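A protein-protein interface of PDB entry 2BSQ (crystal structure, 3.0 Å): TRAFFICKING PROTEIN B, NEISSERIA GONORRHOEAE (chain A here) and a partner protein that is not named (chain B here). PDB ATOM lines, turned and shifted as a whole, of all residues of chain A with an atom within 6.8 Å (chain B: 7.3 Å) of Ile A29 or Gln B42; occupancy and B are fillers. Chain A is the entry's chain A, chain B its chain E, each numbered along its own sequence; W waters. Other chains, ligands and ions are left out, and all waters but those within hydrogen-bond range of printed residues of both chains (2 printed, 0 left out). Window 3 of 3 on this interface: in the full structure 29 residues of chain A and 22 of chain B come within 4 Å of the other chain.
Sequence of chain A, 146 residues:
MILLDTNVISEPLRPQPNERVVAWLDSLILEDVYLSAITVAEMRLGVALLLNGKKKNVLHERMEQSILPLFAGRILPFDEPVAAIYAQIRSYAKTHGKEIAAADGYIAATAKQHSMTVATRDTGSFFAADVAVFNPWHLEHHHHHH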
ATOM      1  N   LEU A  25      33.619  -5.645 -23.479  1.00  0.00           N
ATOM      2  CA  LEU A  25      32.906  -6.446 -22.491  1.00  0.00           C
ATOM      3  C   LEU A  25      31.881  -5.581 -21.764  1.00  0.00           C
ATOM      4  O   LEU A  25      30.801  -6.048 -21.400  1.00  0.00           O
ATOM      5  CB  LEU A  25      33.879  -7.064 -21.480  1.00  0.00           C
ATOM      6  CG  LEU A  25      34.665  -8.316 -21.902  1.00  0.00           C
ATOM      7  CD1 LEU A  25      35.784  -8.572 -20.914  1.00  0.00           C
ATOM      8  CD2 LEU A  25      33.751  -9.516 -21.972  1.00  0.00           C
ATOM      9  N   ASP A  26      32.205  -4.312 -21.558  1.00  0.00           N
ATOM     10  CA  ASP A  26      31.265  -3.439 -20.881  1.00  0.00           C
ATOM     11  C   ASP A  26      30.096  -3.069 -21.765  1.00  0.00           C
ATOM     12  O   ASP A  26      29.015  -2.759 -21.270  1.00  0.00           O
ATOM     13  CB  ASP A  26      31.951  -2.179 -20.385  1.00  0.00           C
ATOM     14  CG  ASP A  26      32.822  -2.441 -19.181  1.00  0.00           C
ATOM     15  OD1 ASP A  26      32.425  -3.277 -18.341  1.00  0.00           O
ATOM     16  OD2 ASP A  26      33.892  -1.812 -19.063  1.00  0.00           O
ATOM     17  N   SER A  27      30.299  -3.106 -23.074  1.00  0.00           N
ATOM     18  CA  SER A  27      29.215  -2.782 -23.982  1.00  0.00           C
ATOM     19  C   SER A  27      28.300  -3.992 -24.082  1.00  0.00           C
ATOM     20  O   SER A  27      27.503  -4.103 -25.018  1.00  0.00           O
ATOM     21  CB  SER A  27      29.751  -2.467 -25.368  1.00  0.00           C
ATOM     22  OG  SER A  27      30.087  -3.661 -26.054  1.00  0.00           O
ATOM     23  N   LEU A  28      28.419  -4.910 -23.129  1.00  0.00           N
ATOM     24  CA  LEU A  28      27.596  -6.107 -23.163  1.00  0.00           C
ATOM     25  C   LEU A  28      26.580  -6.162 -22.044  1.00  0.00           C
ATOM     26  O   LEU A  28      26.745  -5.515 -21.010  1.00  0.00           O
ATOM     27  CB  LEU A  28      28.463  -7.365 -23.096  1.00  0.00           C
ATOM     28  CG  LEU A  28      29.379  -7.710 -24.268  1.00  0.00           C
ATOM     29  CD1 LEU A  28      29.986  -9.066 -24.021  1.00  0.00           C
ATOM     30  CD2 LEU A  28      28.603  -7.715 -25.570  1.00  0.00           C
ATOM     31  N   ILE A  29      25.527  -6.938 -22.277  1.00  0.00           N
ATOM     32  CA  ILE A  29      24.483  -7.143 -21.299  1.00  0.00           C
ATOM     33  C   ILE A  29      24.611  -8.591 -20.824  1.00  0.00           C
ATOM     34  O   ILE A  29      24.320  -9.535 -21.572  1.00  0.00           O
ATOM     35  CB  ILE A  29      23.103  -6.902 -21.919  1.00  0.00           C
ATOM     36  CG1 ILE A  29      22.889  -5.399 -22.070  1.00  0.00           C
ATOM     37  CG2 ILE A  29      22.000  -7.545 -21.058  1.00  0.00           C
ATOM     38  CD1 ILE A  29      21.504  -5.021 -22.477  1.00  0.00           C
ATOM     39  N   LEU A  30      25.053  -8.745 -19.574  1.00  0.00           N
ATOM     40  CA  LEU A  30      25.284 -10.045 -18.950  1.00  0.00           C
ATOM     41  C   LEU A  30      24.401 -11.185 -19.429  1.00  0.00           C
ATOM     42  O   LEU A  30      24.894 -12.186 -19.950  1.00  0.00           O
ATOM     43  CB  LEU A  30      25.170  -9.929 -17.430  1.00  0.00           C
ATOM     44  CG  LEU A  30      25.659 -11.176 -16.678  1.00  0.00           C
ATOM     45  CD1 LEU A  30      27.095 -11.502 -17.082  1.00  0.00           C
ATOM     46  CD2 LEU A  30      25.566 -10.948 -15.176  1.00  0.00           C
ATOM     47  N   GLU A  31      23.099 -11.039 -19.246  1.00  0.00           N
ATOM     48  CA  GLU A  31      22.152 -12.063 -19.656  1.00  0.00           C
ATOM     49  C   GLU A  31      22.349 -12.584 -21.085  1.00  0.00           C
ATOM     50  O   GLU A  31      21.730 -13.566 -21.473  1.00  0.00           O
ATOM     51  CB  GLU A  31      20.738 -11.522 -19.507  1.00  0.00           C
ATOM     52  CG  GLU A  31      20.305 -11.270 -18.059  1.00  0.00           C
ATOM     53  CD  GLU A  31      21.038 -10.113 -17.377  1.00  0.00           C
ATOM     54  OE1 GLU A  31      21.115  -9.011 -17.971  1.00  0.00           O
ATOM     55  OE2 GLU A  31      21.519 -10.302 -16.233  1.00  0.00           O
ATOM     56  N   ASP A  32      23.216 -11.941 -21.861  1.00  0.00           N
ATOM     57  CA  ASP A  32      23.451 -12.337 -23.249  1.00  0.00           C
ATOM     58  C   ASP A  32      24.740 -13.154 -23.431  1.00  0.00           C
ATOM     59  O   ASP A  32      24.927 -13.860 -24.432  1.00  0.00           O
ATOM     60  CB  ASP A  32      23.513 -11.078 -24.110  1.00  0.00           C
ATOM     61  CG  ASP A  32      23.338 -11.368 -25.587  1.00  0.00           C
ATOM     62  OD1 ASP A  32      24.164 -12.112 -26.158  1.00  0.00           O
ATOM     63  OD2 ASP A  32      22.369 -10.850 -26.185  1.00  0.00           O
ATOM     64  N   VAL A  33      25.620 -13.050 -22.444  1.00  0.00           N
ATOM     65  CA  VAL A  33      26.908 -13.721 -22.461  1.00  0.00           C
ATOM     66  C   VAL A  33      26.831 -15.079 -21.787  1.00  0.00           C
ATOM     67  O   VAL A  33      26.284 -15.192 -20.698  1.00  0.00           O
ATOM     68  CB  VAL A  33      27.953 -12.855 -21.731  1.00  0.00           C
ATOM     69  CG1 VAL A  33      29.310 -13.537 -21.733  1.00  0.00           C
ATOM     70  CG2 VAL A  33      28.025 -11.485 -22.381  1.00  0.00           C
ATOM     71  N   ARG A  74      23.725 -19.878 -17.416  1.00  0.00           N
ATOM     72  CA  ARG A  74      24.212 -19.575 -18.744  1.00  0.00           C
ATOM     73  C   ARG A  74      25.573 -20.219 -18.965  1.00  0.00           C
ATOM     74  O   ARG A  74      26.438 -19.670 -19.656  1.00  0.00           O
ATOM     75  CB  ARG A  74      24.283 -18.066 -18.957  1.00  0.00           C
ATOM     76  CG  ARG A  74      22.931 -17.373 -18.854  1.00  0.00           C
ATOM     77  CD  ARG A  74      22.952 -16.006 -19.515  1.00  0.00           C
ATOM     78  NE  ARG A  74      24.098 -15.199 -19.086  1.00  0.00           N
ATOM     79  CZ  ARG A  74      24.300 -14.742 -17.848  1.00  0.00           C
ATOM     80  NH1 ARG A  74      23.431 -14.996 -16.880  1.00  0.00           N
ATOM     81  NH2 ARG A  74      25.392 -14.041 -17.573  1.00  0.00           N
ATOM     82  N   ASP B  36      18.829   4.947 -25.522  1.00  0.00           N
ATOM     83  CA  ASP B  36      19.998   4.874 -24.666  1.00  0.00           C
ATOM     84  C   ASP B  36      19.589   4.769 -23.191  1.00  0.00           C
ATOM     85  O   ASP B  36      20.213   4.056 -22.415  1.00  0.00           O
ATOM     86  CB  ASP B  36      20.881   6.106 -24.903  1.00  0.00           C
ATOM     87  CG  ASP B  36      22.132   5.783 -25.733  1.00  0.00           C
ATOM     88  OD1 ASP B  36      23.083   5.217 -25.145  1.00  0.00           O
ATOM     89  OD2 ASP B  36      22.177   6.075 -26.960  1.00  0.00           O
ATOM     90  N   ASN B  37      18.520   5.454 -22.809  1.00  0.00           N
ATOM     91  CA  ASN B  37      18.072   5.417 -21.421  1.00  0.00           C
ATOM     92  C   ASN B  37      17.626   4.043 -20.937  1.00  0.00           C
ATOM     93  O   ASN B  37      18.020   3.609 -19.858  1.00  0.00           O
ATOM     94  CB  ASN B  37      16.954   6.437 -21.203  1.00  0.00           C
ATOM     95  CG  ASN B  37      17.486   7.840 -20.942  1.00  0.00           C
ATOM     96  OD1 ASN B  37      16.841   8.832 -21.281  1.00  0.00           O
ATOM     97  ND2 ASN B  37      18.656   7.928 -20.324  1.00  0.00           N
ATOM     98  N   ILE B  38      16.813   3.347 -21.716  1.00  0.00           N
ATOM     99  CA  ILE B  38      16.367   2.035 -21.287  1.00  0.00           C
ATOM    100  C   ILE B  38      17.526   1.046 -21.364  1.00  0.00           C
ATOM    101  O   ILE B  38      17.606   0.097 -20.580  1.00  0.00           O
ATOM    102  CB  ILE B  38      15.219   1.524 -22.151  1.00  0.00           C
ATOM    103  CG1 ILE B  38      15.741   1.136 -23.524  1.00  0.00           C
ATOM    104  CG2 ILE B  38      14.157   2.598 -22.292  1.00  0.00           C
ATOM    105  CD1 ILE B  38      14.656   0.645 -24.420  1.00  0.00           C
ATOM    106  N   ALA B  39      18.428   1.279 -22.312  1.00  0.00           N
ATOM    107  CA  ALA B  39      19.585   0.409 -22.482  1.00  0.00           C
ATOM    108  C   ALA B  39      20.406   0.416 -21.206  1.00  0.00           C
ATOM    109  O   ALA B  39      20.774  -0.635 -20.697  1.00  0.00           O
ATOM    110  CB  ALA B  39      20.429   0.882 -23.650  1.00  0.00           C
ATOM    111  N   LYS B  40      20.680   1.610 -20.690  1.00  0.00           N
ATOM    112  CA  LYS B  40      21.459   1.770 -19.465  1.00  0.00           C
ATOM    113  C   LYS B  40      20.736   1.092 -18.312  1.00  0.00           C
ATOM    114  O   LYS B  40      21.346   0.722 -17.302  1.00  0.00           O
ATOM    115  CB  LYS B  40      21.644   3.254 -19.144  1.00  0.00           C
ATOM    116  CG  LYS B  40      22.798   3.566 -18.187  1.00  0.00           C
ATOM    117  CD  LYS B  40      22.363   4.502 -17.048  1.00  0.00           C
ATOM    118  CE  LYS B  40      21.411   5.625 -17.527  1.00  0.00           C
ATOM    119  NZ  LYS B  40      21.955   6.507 -18.614  1.00  0.00           N
ATOM    120  N   ALA B  41      19.426   0.946 -18.466  1.00  0.00           N
ATOM    121  CA  ALA B  41      18.619   0.291 -17.460  1.00  0.00           C
ATOM    122  C   ALA B  41      18.890  -1.219 -17.529  1.00  0.00           C
ATOM    123  O   ALA B  41      19.044  -1.874 -16.498  1.00  0.00           O
ATOM    124  CB  ALA B  41      17.164   0.590 -17.707  1.00  0.00           C
ATOM    125  N   GLN B  42      18.958  -1.772 -18.741  1.00  0.00           N
ATOM    126  CA  GLN B  42      19.242  -3.199 -18.913  1.00  0.00           C
ATOM    127  C   GLN B  42      20.634  -3.535 -18.377  1.00  0.00           C
ATOM    128  O   GLN B  42      20.897  -4.660 -17.960  1.00  0.00           O
ATOM    129  CB  GLN B  42      19.193  -3.600 -20.392  1.00  0.00           C
ATOM    130  CG  GLN B  42      17.806  -3.750 -21.003  1.00  0.00           C
ATOM    131  CD  GLN B  42      17.079  -5.030 -20.589  1.00  0.00           C
ATOM    132  OE1 GLN B  42      17.539  -6.145 -20.855  1.00  0.00           O
ATOM    133  NE2 GLN B  42      15.930  -4.868 -19.943  1.00  0.00           N
ATOM    134  N   GLN B  43      21.525  -2.553 -18.409  1.00  0.00           N
ATOM    135  CA  GLN B  43      22.897  -2.727 -17.948  1.00  0.00           C
ATOM    136  C   GLN B  43      22.952  -2.947 -16.442  1.00  0.00           C
ATOM    137  O   GLN B  43      23.226  -2.015 -15.683  1.00  0.00           O
ATOM    138  CB  GLN B  43      23.724  -1.487 -18.300  1.00  0.00           C
ATOM    139  CG  GLN B  43      25.240  -1.662 -18.200  1.00  0.00           C
ATOM    140  CD  GLN B  43      25.805  -2.439 -19.371  1.00  0.00           C
ATOM    141  OE1 GLN B  43      27.014  -2.485 -19.577  1.00  0.00           O
ATOM    142  NE2 GLN B  43      24.926  -3.057 -20.145  1.00  0.00           N
ATOM    143  N   THR B  44      22.692  -4.177 -16.014  1.00  0.00           N
ATOM    144  CA  THR B  44      22.720  -4.508 -14.597  1.00  0.00           C
ATOM    145  C   THR B  44      24.165  -4.535 -14.111  1.00  0.00           C
ATOM    146  O   THR B  44      24.470  -4.115 -12.995  1.00  0.00           O
ATOM    147  CB  THR B  44      22.074  -5.884 -14.333  1.00  0.00           C
ATOM    148  OG1 THR B  44      20.712  -5.868 -14.779  1.00  0.00           O
ATOM    149  CG2 THR B  44      22.100  -6.212 -12.850  1.00  0.00           C
ATOM    150  N   VAL B  45      25.058  -5.035 -14.955  1.00  0.00           N
ATOM    151  CA  VAL B  45      26.473  -5.102 -14.603  1.00  0.00           C
ATOM    152  C   VAL B  45      27.371  -4.960 -15.829  1.00  0.00           C
ATOM    153  O   VAL B  45      26.999  -5.333 -16.945  1.00  0.00           O
ATOM    154  CB  VAL B  45      26.798  -6.423 -13.856  1.00  0.00           C
ATOM    155  CG1 VAL B  45      26.319  -6.334 -12.417  1.00  0.00           C
ATOM    156  CG2 VAL B  45      26.114  -7.589 -14.540  1.00  0.00           C
ATOM    157  N   LEU B  47      30.455  -6.357 -17.250  1.00  0.00           N
ATOM    158  CA  LEU B  47      31.410  -7.445 -17.148  1.00  0.00           C
ATOM    159  C   LEU B  47      32.873  -7.033 -17.274  1.00  0.00           C
ATOM    160  O   LEU B  47      33.701  -7.425 -16.453  1.00  0.00           O
ATOM    161  CB  LEU B  47      31.074  -8.518 -18.179  1.00  0.00           C
ATOM    162  CG  LEU B  47      31.703  -9.868 -17.849  1.00  0.00           C
ATOM    163  CD1 LEU B  47      31.230 -10.337 -16.470  1.00  0.00           C
ATOM    164  CD2 LEU B  47      31.345 -10.871 -18.931  1.00  0.00           C
HETATM  165  O   HOH W   1      25.102  -6.428 -18.172  1.00  0.00           O
HETATM  166  O   HOH W   2      22.649  -7.278 -16.777  1.00  0.00           O
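Water W1 lies within hydrogen-bond range of O of Val B45 (2.5 Å), N of Leu A30 (2.7 Å) and O of Leu A28 (3.4 Å). Water W2 lies within hydrogen-bond range of the side-chain carboxylate of Glu A31 (2.6 Å), the side-chain hydroxyl of Thr B44 (3.1 Å) and the backbone carbonyl oxygen of Gln B42 (3.4 Å).
Among the printed residues, pairs that only touch across the chains: Ile A29 with Gln B42, Leu A30 with Val B45, Ile A29 with Gln B43 and Asp A26 with Leu B47.
Of the printed residues of chain B, Asp A26 touches Gln B43 and Leu B47. Ser A27 touches none of the printed residues of chain B. Of chain B, only Gln B42 (3.4 Å) and Gln B43 (3.7 Å) come within 4 Å of Ile A29. Of the printed residues of chain B, Leu A30 touches Val B45 (3.5 Å). Gln B42 touches just one residue of chain A: Ile A29. Of the printed residues of chain A, Leu B47 touches Asp A26. The nearest residue of chain B that does not touch Ile A29 is Ala B39 (4.8 Å). The nearest residue of chain A that does not touch Gln B42 is Glu A31 (4.4 Å).
NH2 of Arg A74 lies close to O of Leu A30. OG1 of Thr B44 is in hydrogen-bond range of O of Gln B42, 3.4 Å away.
Among the printed residues, 6 pairs touch across the chains. Among the printed residues, no Asp or Glu carboxylate lies within 4 Å of a Lys or Arg side-chain nitrogen of the other chain.
The side-chain amide oxygen (OE1) of Gln B43 sits close to the backbone carbonyl oxygen (O) of Asp A26. The backbone carbonyl oxygen (O) of Leu A28 is in hydrogen-bond range of the side-chain amide nitrogen (NE2) of Gln B43, 3.2 Å away.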
